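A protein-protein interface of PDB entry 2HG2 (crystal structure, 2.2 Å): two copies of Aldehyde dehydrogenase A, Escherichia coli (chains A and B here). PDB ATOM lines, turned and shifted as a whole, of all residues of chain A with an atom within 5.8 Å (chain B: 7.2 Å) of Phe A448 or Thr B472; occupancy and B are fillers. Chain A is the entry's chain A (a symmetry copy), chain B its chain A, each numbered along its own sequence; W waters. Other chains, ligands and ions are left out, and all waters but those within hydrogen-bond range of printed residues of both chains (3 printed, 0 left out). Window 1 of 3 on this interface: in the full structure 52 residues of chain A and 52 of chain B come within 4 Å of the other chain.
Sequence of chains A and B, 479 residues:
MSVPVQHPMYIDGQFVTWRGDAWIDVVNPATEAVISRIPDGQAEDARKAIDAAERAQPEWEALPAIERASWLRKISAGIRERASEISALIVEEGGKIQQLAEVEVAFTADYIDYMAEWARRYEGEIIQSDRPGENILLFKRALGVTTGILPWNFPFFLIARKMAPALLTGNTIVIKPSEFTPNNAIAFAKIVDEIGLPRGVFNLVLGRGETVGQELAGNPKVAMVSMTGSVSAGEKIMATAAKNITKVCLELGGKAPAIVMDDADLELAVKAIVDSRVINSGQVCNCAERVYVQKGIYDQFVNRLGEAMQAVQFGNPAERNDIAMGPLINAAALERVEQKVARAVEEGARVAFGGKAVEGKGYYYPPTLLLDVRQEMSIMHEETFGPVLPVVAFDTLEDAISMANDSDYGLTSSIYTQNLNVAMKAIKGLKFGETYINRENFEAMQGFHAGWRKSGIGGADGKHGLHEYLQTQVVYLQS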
ATOM      1  N   PHE A 432      28.447 -10.951  32.468  1.00  0.00           N
ATOM      2  CA  PHE A 432      29.072 -10.195  31.391  1.00  0.00           C
ATOM      3  C   PHE A 432      28.421 -10.447  30.043  1.00  0.00           C
ATOM      4  O   PHE A 432      27.743 -11.450  29.855  1.00  0.00           O
ATOM      5  CB  PHE A 432      30.564 -10.546  31.305  1.00  0.00           C
ATOM      6  CG  PHE A 432      31.359 -10.073  32.481  1.00  0.00           C
ATOM      7  CD1 PHE A 432      31.259 -10.718  33.711  1.00  0.00           C
ATOM      8  CD2 PHE A 432      32.156  -8.934  32.380  1.00  0.00           C
ATOM      9  CE1 PHE A 432      31.938 -10.227  34.830  1.00  0.00           C
ATOM     10  CE2 PHE A 432      32.836  -8.438  33.490  1.00  0.00           C
ATOM     11  CZ  PHE A 432      32.727  -9.085  34.718  1.00  0.00           C
ATOM     12  N   GLY A 433      28.635  -9.525  29.110  1.00  0.00           N
ATOM     13  CA  GLY A 433      28.076  -9.667  27.778  1.00  0.00           C
ATOM     14  C   GLY A 433      28.813 -10.735  26.990  1.00  0.00           C
ATOM     15  O   GLY A 433      28.289 -11.265  26.005  1.00  0.00           O
ATOM     16  N   GLU A 434      30.030 -11.053  27.425  1.00  0.00           N
ATOM     17  CA  GLU A 434      30.847 -12.063  26.758  1.00  0.00           C
ATOM     18  C   GLU A 434      31.723 -12.823  27.748  1.00  0.00           C
ATOM     19  O   GLU A 434      32.242 -12.250  28.702  1.00  0.00           O
ATOM     20  CB  GLU A 434      31.771 -11.422  25.710  1.00  0.00           C
ATOM     21  CG  GLU A 434      31.111 -10.442  24.763  1.00  0.00           C
ATOM     22  CD  GLU A 434      32.107  -9.807  23.801  1.00  0.00           C
ATOM     23  OE1 GLU A 434      33.221  -9.456  24.245  1.00  0.00           O
ATOM     24  OE2 GLU A 434      31.770  -9.647  22.607  1.00  0.00           O
ATOM     25  N   ALA A 444      33.673 -12.147  17.459  1.00  0.00           N
ATOM     26  CA  ALA A 444      33.424 -12.536  16.075  1.00  0.00           C
ATOM     27  C   ALA A 444      32.398 -11.579  15.455  1.00  0.00           C
ATOM     28  O   ALA A 444      31.543 -11.033  16.159  1.00  0.00           O
ATOM     29  CB  ALA A 444      32.908 -13.980  16.020  1.00  0.00           C
ATOM     30  N   GLN A 446      29.923 -12.295  13.711  1.00  0.00           N
ATOM     31  CA  GLN A 446      28.581 -12.873  13.807  1.00  0.00           C
ATOM     32  C   GLN A 446      28.117 -13.007  15.268  1.00  0.00           C
ATOM     33  O   GLN A 446      27.072 -13.590  15.538  1.00  0.00           O
ATOM     34  CB  GLN A 446      28.515 -14.252  13.126  1.00  0.00           C
ATOM     35  CG  GLN A 446      29.368 -15.328  13.785  1.00  0.00           C
ATOM     36  CD  GLN A 446      30.746 -15.464  13.161  1.00  0.00           C
ATOM     37  OE1 GLN A 446      31.432 -14.470  12.919  1.00  0.00           O
ATOM     38  NE2 GLN A 446      31.162 -16.704  12.903  1.00  0.00           N
ATOM     39  N   GLY A 447      28.906 -12.488  16.204  1.00  0.00           N
ATOM     40  CA  GLY A 447      28.527 -12.553  17.606  1.00  0.00           C
ATOM     41  C   GLY A 447      27.716 -11.314  17.966  1.00  0.00           C
ATOM     42  O   GLY A 447      27.068 -10.726  17.101  1.00  0.00           O
ATOM     43  N   PHE A 448      27.739 -10.917  19.234  1.00  0.00           N
ATOM     44  CA  PHE A 448      27.012  -9.729  19.677  1.00  0.00           C
ATOM     45  C   PHE A 448      27.812  -9.126  20.825  1.00  0.00           C
ATOM     46  O   PHE A 448      27.818  -9.644  21.945  1.00  0.00           O
ATOM     47  CB  PHE A 448      25.592 -10.084  20.138  1.00  0.00           C
ATOM     48  CG  PHE A 448      24.729  -8.878  20.462  1.00  0.00           C
ATOM     49  CD1 PHE A 448      24.737  -7.747  19.638  1.00  0.00           C
ATOM     50  CD2 PHE A 448      23.878  -8.892  21.559  1.00  0.00           C
ATOM     51  CE1 PHE A 448      23.903  -6.645  19.905  1.00  0.00           C
ATOM     52  CE2 PHE A 448      23.032  -7.796  21.846  1.00  0.00           C
ATOM     53  CZ  PHE A 448      23.050  -6.670  21.010  1.00  0.00           C
ATOM     54  N   HIS A 449      28.508  -8.039  20.515  1.00  0.00           N
ATOM     55  CA  HIS A 449      29.352  -7.322  21.459  1.00  0.00           C
ATOM     56  C   HIS A 449      28.477  -6.286  22.155  1.00  0.00           C
ATOM     57  O   HIS A 449      28.278  -5.184  21.634  1.00  0.00           O
ATOM     58  CB  HIS A 449      30.478  -6.643  20.679  1.00  0.00           C
ATOM     59  CG  HIS A 449      31.595  -6.130  21.529  1.00  0.00           C
ATOM     60  ND1 HIS A 449      32.401  -6.958  22.284  1.00  0.00           N
ATOM     61  CD2 HIS A 449      32.066  -4.874  21.717  1.00  0.00           C
ATOM     62  CE1 HIS A 449      33.318  -6.234  22.899  1.00  0.00           C
ATOM     63  NE2 HIS A 449      33.137  -4.966  22.571  1.00  0.00           N
ATOM     64  N   ALA A 450      27.946  -6.647  23.321  1.00  0.00           N
ATOM     65  CA  ALA A 450      27.060  -5.763  24.083  1.00  0.00           C
ATOM     66  C   ALA A 450      27.376  -5.844  25.574  1.00  0.00           C
ATOM     67  O   ALA A 450      27.350  -6.919  26.169  1.00  0.00           O
ATOM     68  CB  ALA A 450      25.602  -6.148  23.832  1.00  0.00           C
ATOM     69  N   TRP A 452      27.126  -5.182  29.747  1.00  0.00           N
ATOM     70  CA  TRP A 452      26.206  -5.133  30.867  1.00  0.00           C
ATOM     71  C   TRP A 452      26.570  -3.924  31.728  1.00  0.00           C
ATOM     72  O   TRP A 452      27.658  -3.356  31.588  1.00  0.00           O
ATOM     73  CB  TRP A 452      26.345  -6.407  31.698  1.00  0.00           C
ATOM     74  CG  TRP A 452      25.767  -7.652  31.067  1.00  0.00           C
ATOM     75  CD1 TRP A 452      25.655  -7.931  29.734  1.00  0.00           C
ATOM     76  CD2 TRP A 452      25.239  -8.791  31.761  1.00  0.00           C
ATOM     77  NE1 TRP A 452      25.085  -9.172  29.555  1.00  0.00           N
ATOM     78  CE2 TRP A 452      24.820  -9.721  30.783  1.00  0.00           C
ATOM     79  CE3 TRP A 452      25.073  -9.111  33.116  1.00  0.00           C
ATOM     80  CZ2 TRP A 452      24.249 -10.953  31.115  1.00  0.00           C
ATOM     81  CZ3 TRP A 452      24.502 -10.342  33.446  1.00  0.00           C
ATOM     82  CH2 TRP A 452      24.098 -11.245  32.446  1.00  0.00           C
ATOM     83  N   GLY A 458      22.464  -1.383  24.351  1.00  0.00           N
ATOM     84  CA  GLY A 458      22.379  -1.914  23.005  1.00  0.00           C
ATOM     85  C   GLY A 458      23.695  -2.630  22.715  1.00  0.00           C
ATOM     86  O   GLY A 458      24.403  -3.036  23.640  1.00  0.00           O
ATOM     87  N   GLY A 459      24.043  -2.781  21.444  1.00  0.00           N
ATOM     88  CA  GLY A 459      25.286  -3.460  21.127  1.00  0.00           C
ATOM     89  C   GLY A 459      25.612  -3.449  19.651  1.00  0.00           C
ATOM     90  O   GLY A 459      24.922  -2.800  18.862  1.00  0.00           O
ATOM     91  N   ALA A 460      26.656  -4.191  19.281  1.00  0.00           N
ATOM     92  CA  ALA A 460      27.096  -4.258  17.893  1.00  0.00           C
ATOM     93  C   ALA A 460      27.443  -5.665  17.422  1.00  0.00           C
ATOM     94  O   ALA A 460      27.652  -6.575  18.225  1.00  0.00           O
ATOM     95  CB  ALA A 460      28.298  -3.343  17.698  1.00  0.00           C
ATOM     96  N   ASP A 461      27.497  -5.815  16.101  1.00  0.00           N
ATOM     97  CA  ASP A 461      27.834  -7.066  15.426  1.00  0.00           C
ATOM     98  C   ASP A 461      26.672  -8.048  15.322  1.00  0.00           C
ATOM     99  O   ASP A 461      25.696  -7.987  16.084  1.00  0.00           O
ATOM    100  CB  ASP A 461      29.007  -7.788  16.117  1.00  0.00           C
ATOM    101  CG  ASP A 461      30.193  -6.870  16.413  1.00  0.00           C
ATOM    102  OD1 ASP A 461      30.304  -5.786  15.806  1.00  0.00           O
ATOM    103  OD2 ASP A 461      31.033  -7.250  17.258  1.00  0.00           O
ATOM    104  N   GLY A 462      26.800  -8.953  14.357  1.00  0.00           N
ATOM    105  CA  GLY A 462      25.811  -9.988  14.146  1.00  0.00           C
ATOM    106  C   GLY A 462      24.401  -9.518  13.903  1.00  0.00           C
ATOM    107  O   GLY A 462      24.153  -8.339  13.653  1.00  0.00           O
ATOM    108  N   HIS A 464      21.822  -9.301  16.024  1.00  0.00           N
ATOM    109  CA  HIS A 464      21.331  -8.373  17.035  1.00  0.00           C
ATOM    110  C   HIS A 464      21.898  -6.984  16.831  1.00  0.00           C
ATOM    111  O   HIS A 464      21.211  -5.990  17.068  1.00  0.00           O
ATOM    112  CB  HIS A 464      21.664  -8.894  18.433  1.00  0.00           C
ATOM    113  CG  HIS A 464      21.038 -10.221  18.727  1.00  0.00           C
ATOM    114  ND1 HIS A 464      19.686 -10.369  18.954  1.00  0.00           N
ATOM    115  CD2 HIS A 464      21.563 -11.468  18.750  1.00  0.00           C
ATOM    116  CE1 HIS A 464      19.405 -11.651  19.101  1.00  0.00           C
ATOM    117  NE2 HIS A 464      20.526 -12.340  18.980  1.00  0.00           N
ATOM    118  N   GLY A 465      23.151  -6.910  16.398  1.00  0.00           N
ATOM    119  CA  GLY A 465      23.743  -5.609  16.142  1.00  0.00           C
ATOM    120  C   GLY A 465      23.020  -4.942  14.983  1.00  0.00           C
ATOM    121  O   GLY A 465      22.752  -3.741  15.011  1.00  0.00           O
ATOM    122  N   GLU A 468      19.743  -3.227  15.923  1.00  0.00           N
ATOM    123  CA  GLU A 468      19.780  -1.958  16.652  1.00  0.00           C
ATOM    124  C   GLU A 468      19.372  -0.840  15.689  1.00  0.00           C
ATOM    125  O   GLU A 468      18.914   0.223  16.115  1.00  0.00           O
ATOM    126  CB  GLU A 468      21.194  -1.647  17.162  1.00  0.00           C
ATOM    127  CG  GLU A 468      21.682  -2.506  18.303  1.00  0.00           C
ATOM    128  CD  GLU A 468      20.853  -2.316  19.548  1.00  0.00           C
ATOM    129  OE1 GLU A 468      20.532  -1.150  19.862  1.00  0.00           O
ATOM    130  OE2 GLU A 468      20.527  -3.324  20.213  1.00  0.00           O
ATOM    131  N   GLU B 125      20.715 -18.570  21.439  1.00  0.00           N
ATOM    132  CA  GLU B 125      21.107 -19.094  20.143  1.00  0.00           C
ATOM    133  C   GLU B 125      22.485 -19.709  20.116  1.00  0.00           C
ATOM    134  O   GLU B 125      23.341 -19.403  20.943  1.00  0.00           O
ATOM    135  CB  GLU B 125      21.033 -17.965  19.119  1.00  0.00           C
ATOM    136  CG  GLU B 125      19.693 -17.249  19.095  1.00  0.00           C
ATOM    137  CD  GLU B 125      19.816 -15.799  18.662  1.00  0.00           C
ATOM    138  OE1 GLU B 125      20.694 -15.092  19.197  1.00  0.00           O
ATOM    139  OE2 GLU B 125      19.027 -15.360  17.797  1.00  0.00           O
ATOM    140  N   ILE B 127      25.546 -20.106  17.535  1.00  0.00           N
ATOM    141  CA  ILE B 127      26.085 -19.528  16.311  1.00  0.00           C
ATOM    142  C   ILE B 127      27.322 -20.219  15.754  1.00  0.00           C
ATOM    143  O   ILE B 127      28.247 -20.554  16.498  1.00  0.00           O
ATOM    144  CB  ILE B 127      26.413 -18.039  16.564  1.00  0.00           C
ATOM    145  CG1 ILE B 127      25.173 -17.335  17.134  1.00  0.00           C
ATOM    146  CG2 ILE B 127      26.885 -17.370  15.286  1.00  0.00           C
ATOM    147  CD1 ILE B 127      25.441 -15.927  17.684  1.00  0.00           C
ATOM    148  N   ILE B 136      29.863 -21.052  19.696  1.00  0.00           N
ATOM    149  CA  ILE B 136      29.514 -19.720  20.160  1.00  0.00           C
ATOM    150  C   ILE B 136      28.092 -19.877  20.706  1.00  0.00           C
ATOM    151  O   ILE B 136      27.157 -20.159  19.951  1.00  0.00           O
ATOM    152  CB  ILE B 136      29.526 -18.696  19.016  1.00  0.00           C
ATOM    153  CG1 ILE B 136      30.928 -18.619  18.399  1.00  0.00           C
ATOM    154  CG2 ILE B 136      29.101 -17.335  19.539  1.00  0.00           C
ATOM    155  CD1 ILE B 136      31.024 -17.683  17.190  1.00  0.00           C
ATOM    156  N   LEU B 138      24.979 -18.106  22.692  1.00  0.00           N
ATOM    157  CA  LEU B 138      24.400 -16.842  23.123  1.00  0.00           C
ATOM    158  C   LEU B 138      23.214 -17.102  24.053  1.00  0.00           C
ATOM    159  O   LEU B 138      22.162 -17.547  23.613  1.00  0.00           O
ATOM    160  CB  LEU B 138      23.966 -16.037  21.896  1.00  0.00           C
ATOM    161  CG  LEU B 138      23.290 -14.687  22.117  1.00  0.00           C
ATOM    162  CD1 LEU B 138      23.550 -13.777  20.909  1.00  0.00           C
ATOM    163  CD2 LEU B 138      21.786 -14.900  22.343  1.00  0.00           C
ATOM    164  N   PHE B 139      23.394 -16.845  25.345  1.00  0.00           N
ATOM    165  CA  PHE B 139      22.318 -17.072  26.308  1.00  0.00           C
ATOM    166  C   PHE B 139      21.534 -15.783  26.587  1.00  0.00           C
ATOM    167  O   PHE B 139      22.060 -14.675  26.440  1.00  0.00           O
ATOM    168  CB  PHE B 139      22.865 -17.590  27.647  1.00  0.00           C
ATOM    169  CG  PHE B 139      23.632 -18.882  27.561  1.00  0.00           C
ATOM    170  CD1 PHE B 139      24.963 -18.898  27.155  1.00  0.00           C
ATOM    171  CD2 PHE B 139      23.044 -20.084  27.963  1.00  0.00           C
ATOM    172  CE1 PHE B 139      25.703 -20.089  27.160  1.00  0.00           C
ATOM    173  CE2 PHE B 139      23.772 -21.276  27.969  1.00  0.00           C
ATOM    174  CZ  PHE B 139      25.108 -21.281  27.569  1.00  0.00           C
ATOM    175  N   LYS B 140      20.279 -15.938  26.997  1.00  0.00           N
ATOM    176  CA  LYS B 140      19.423 -14.800  27.331  1.00  0.00           C
ATOM    177  C   LYS B 140      19.297 -14.769  28.855  1.00  0.00           C
ATOM    178  O   LYS B 140      18.710 -15.672  29.449  1.00  0.00           O
ATOM    179  CB  LYS B 140      18.040 -14.969  26.699  1.00  0.00           C
ATOM    180  CG  LYS B 140      18.022 -14.944  25.188  1.00  0.00           C
ATOM    181  CD  LYS B 140      18.273 -13.551  24.653  1.00  0.00           C
ATOM    182  CE  LYS B 140      18.213 -13.537  23.132  1.00  0.00           C
ATOM    183  NZ  LYS B 140      16.936 -14.106  22.608  1.00  0.00           N
ATOM    184  N   ARG B 141      19.840 -13.728  29.479  1.00  0.00           N
ATOM    185  CA  ARG B 141      19.819 -13.601  30.932  1.00  0.00           C
ATOM    186  C   ARG B 141      18.971 -12.420  31.403  1.00  0.00           C
ATOM    187  O   ARG B 141      18.675 -11.505  30.635  1.00  0.00           O
ATOM    188  CB  ARG B 141      21.247 -13.402  31.467  1.00  0.00           C
ATOM    189  CG  ARG B 141      22.305 -14.344  30.918  1.00  0.00           C
ATOM    190  CD  ARG B 141      22.097 -15.776  31.377  1.00  0.00           C
ATOM    191  NE  ARG B 141      23.307 -16.577  31.193  1.00  0.00           N
ATOM    192  CZ  ARG B 141      23.353 -17.905  31.293  1.00  0.00           C
ATOM    193  NH1 ARG B 141      22.256 -18.598  31.573  1.00  0.00           N
ATOM    194  NH2 ARG B 141      24.499 -18.546  31.110  1.00  0.00           N
ATOM    195  N   ALA B 142      18.609 -12.444  32.685  1.00  0.00           N
ATOM    196  CA  ALA B 142      17.830 -11.378  33.300  1.00  0.00           C
ATOM    197  C   ALA B 142      18.722 -10.145  33.439  1.00  0.00           C
ATOM    198  O   ALA B 142      19.948 -10.255  33.452  1.00  0.00           O
ATOM    199  CB  ALA B 142      17.343 -11.817  34.683  1.00  0.00           C
ATOM    200  N   LEU B 143      18.107  -8.975  33.532  1.00  0.00           N
ATOM    201  CA  LEU B 143      18.853  -7.738  33.696  1.00  0.00           C
ATOM    202  C   LEU B 143      19.259  -7.635  35.160  1.00  0.00           C
ATOM    203  O   LEU B 143      20.378  -7.256  35.476  1.00  0.00           O
ATOM    204  CB  LEU B 143      17.986  -6.527  33.321  1.00  0.00           C
ATOM    205  CG  LEU B 143      17.329  -6.529  31.933  1.00  0.00           C
ATOM    206  CD1 LEU B 143      16.681  -5.168  31.671  1.00  0.00           C
ATOM    207  CD2 LEU B 143      18.384  -6.818  30.862  1.00  0.00           C
ATOM    208  N   LEU B 470      15.497  -8.895  28.887  1.00  0.00           N
ATOM    209  CA  LEU B 470      16.571  -9.871  28.755  1.00  0.00           C
ATOM    210  C   LEU B 470      17.791  -9.218  28.132  1.00  0.00           C
ATOM    211  O   LEU B 470      17.675  -8.244  27.405  1.00  0.00           O
ATOM    212  CB  LEU B 470      16.122 -11.037  27.868  1.00  0.00           C
ATOM    213  CG  LEU B 470      15.039 -11.949  28.448  1.00  0.00           C
ATOM    214  CD1 LEU B 470      14.442 -12.811  27.348  1.00  0.00           C
ATOM    215  CD2 LEU B 470      15.637 -12.809  29.550  1.00  0.00           C
ATOM    216  N   GLN B 471      18.966  -9.748  28.440  1.00  0.00           N
ATOM    217  CA  GLN B 471      20.190  -9.237  27.853  1.00  0.00           C
ATOM    218  C   GLN B 471      20.990 -10.478  27.497  1.00  0.00           C
ATOM    219  O   GLN B 471      20.781 -11.551  28.070  1.00  0.00           O
ATOM    220  CB  GLN B 471      20.949  -8.327  28.829  1.00  0.00           C
ATOM    221  CG  GLN B 471      21.485  -9.001  30.069  1.00  0.00           C
ATOM    222  CD  GLN B 471      22.015  -7.993  31.064  1.00  0.00           C
ATOM    223  OE1 GLN B 471      22.359  -6.866  30.698  1.00  0.00           O
ATOM    224  NE2 GLN B 471      22.092  -8.392  32.328  1.00  0.00           N
ATOM    225  N   THR B 472      21.903 -10.340  26.551  1.00  0.00           N
ATOM    226  CA  THR B 472      22.665 -11.483  26.099  1.00  0.00           C
ATOM    227  C   THR B 472      24.024 -11.696  26.731  1.00  0.00           C
ATOM    228  O   THR B 472      24.681 -10.754  27.176  1.00  0.00           O
ATOM    229  CB  THR B 472      22.862 -11.428  24.567  1.00  0.00           C
ATOM    230  OG1 THR B 472      23.730 -10.337  24.234  1.00  0.00           O
ATOM    231  CG2 THR B 472      21.533 -11.211  23.867  1.00  0.00           C
ATOM    232  N   GLN B 473      24.414 -12.965  26.789  1.00  0.00           N
ATOM    233  CA  GLN B 473      25.730 -13.362  27.263  1.00  0.00           C
ATOM    234  C   GLN B 473      26.246 -14.306  26.170  1.00  0.00           C
ATOM    235  O   GLN B 473      25.732 -15.413  25.995  1.00  0.00           O
ATOM    236  CB  GLN B 473      25.690 -14.109  28.598  1.00  0.00           C
ATOM    237  CG  GLN B 473      27.045 -14.763  28.898  1.00  0.00           C
ATOM    238  CD  GLN B 473      27.055 -15.632  30.137  1.00  0.00           C
ATOM    239  OE1 GLN B 473      26.032 -16.197  30.524  1.00  0.00           O
ATOM    240  NE2 GLN B 473      28.228 -15.766  30.755  1.00  0.00           N
ATOM    241  N   VAL B 474      27.242 -13.848  25.420  1.00  0.00           N
ATOM    242  CA  VAL B 474      27.815 -14.652  24.349  1.00  0.00           C
ATOM    243  C   VAL B 474      29.037 -15.386  24.876  1.00  0.00           C
ATOM    244  O   VAL B 474      30.022 -14.762  25.278  1.00  0.00           O
ATOM    245  CB  VAL B 474      28.218 -13.767  23.146  1.00  0.00           C
ATOM    246  CG1 VAL B 474      28.831 -14.618  22.044  1.00  0.00           C
ATOM    247  CG2 VAL B 474      27.002 -13.029  22.622  1.00  0.00           C
ATOM    248  N   TYR B 476      32.118 -17.916  24.125  1.00  0.00           N
ATOM    249  CA  TYR B 476      32.968 -18.489  23.085  1.00  0.00           C
ATOM    250  C   TYR B 476      33.698 -19.664  23.733  1.00  0.00           C
ATOM    251  O   TYR B 476      34.724 -19.495  24.399  1.00  0.00           O
ATOM    252  CB  TYR B 476      33.977 -17.455  22.568  1.00  0.00           C
ATOM    253  CG  TYR B 476      33.359 -16.293  21.801  1.00  0.00           C
ATOM    254  CD1 TYR B 476      32.788 -15.207  22.471  1.00  0.00           C
ATOM    255  CD2 TYR B 476      33.356 -16.278  20.402  1.00  0.00           C
ATOM    256  CE1 TYR B 476      32.237 -14.136  21.770  1.00  0.00           C
ATOM    257  CE2 TYR B 476      32.800 -15.209  19.690  1.00  0.00           C
ATOM    258  CZ  TYR B 476      32.246 -14.141  20.383  1.00  0.00           C
ATOM    259  OH  TYR B 476      31.715 -13.076  19.691  1.00  0.00           O
HETATM  260  O   HOH W   1      24.711  -7.834  26.534  1.00  0.00           O
HETATM  261  O   HOH W   2      26.505  -9.875  24.325  1.00  0.00           O
HETATM  262  O   HOH W   3      30.441 -11.002  20.665  1.00  0.00           O
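O of Thr B472 lies within hydrogen-bond range of NE1 of Trp A452, at 2.9 Å. The backbone carbonyl oxygen (O) of Gly A433 is in hydrogen-bond range of the backbone NH (N) of Val B474 (2.8 Å). The side-chain hydroxyl of Tyr B476 lies within hydrogen-bond range of the backbone NH of Ala A444. OE1 of Glu B125 sits at hydrogen-bond distance from NE2 of His A464.
Of the 18 printed residues of chain A, 9 touch a printed residue of chain B. Among the printed residues, 15 pairs touch across the chains.
No position is printed for both chains. Of the 15 pairs that touch across the chains among the printed residues, none has its exchanged pair printed and touching as well.
Among the printed residues, pairs that only touch across the chains: Phe A448 with Thr B472 (3.0 Å), Trp A452 with Gln B471 (3.2 Å), Glu A434 with Val B474 (3.2 Å), Phe A432 with Gln B473 (3.5 Å), Gly A433 with Gln B473 (3.5 Å), Phe A448 with Val B474 (3.5 Å), Gln A446 with Ile B127 (3.5 Å), Gly A433 with Thr B472 (3.6 Å), Trp A452 with Arg B141 (3.7 Å), His A464 with Leu B138 (3.7 Å) and Gly A447 with Tyr B476 (3.8 Å).
The backbone carbonyl oxygen (O) of Ile B136 is in hydrogen-bond range of the backbone NH (N) of Ile B127, at 2.9 Å. NE of Arg B141 lies within hydrogen-bond range of OE1 of Gln B473, at 2.8 Å. The backbone carbonyl oxygen of Ala B142 is in hydrogen-bond range of the side-chain amide nitrogen of Gln B471 (3.1 Å). The backbone NH (N) of Leu B138 is in hydrogen-bond range of the backbone carbonyl oxygen (O) of Glu B125, 2.7 Å away. N of Arg B141 lies within hydrogen-bond range of O of Gln B471 (2.8 Å). N of Phe B139 lies within hydrogen-bond range of O of Gln B473 (2.8 Å).
Of the printed residues of chain B, Gly A447 touches Tyr B476. Of the printed residues of chain B, Phe A448 touches Thr B472 and Val B474. Printed residues of chain B within 4 Å of His A464: Glu B125 and Leu B138. Printed residues of chain A within 4 Å of Leu B138: His A464. Thr B472 touches just these residues of chain A: Gly A433 (3.6 Å), Phe A448 (3.0 Å) and Trp A452 (2.9 Å). The nearest residue of chain B that does not touch Phe A448 is Leu B138 (4.3 Å). The nearest printed residue of chain B that does not touch Glu A434 is Tyr B476 (4.5 Å).
Water W3 lies within hydrogen-bond range of OH of Tyr B476 (2.6 Å), OE2 of Glu A434 (2.7 Å) and N of Phe A448 (3.1 Å). Water W2 lies within hydrogen-bond range of O of Phe A448 (2.7 Å), OG1 of Thr B472 (2.8 Å) and O of Gly A433 (2.8 Å). Water W1 lies within hydrogen-bond range of O of Ala A450 (2.8 Å), O of Thr B472 (3.0 Å) and NE1 of Trp A452 (3.3 Å).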
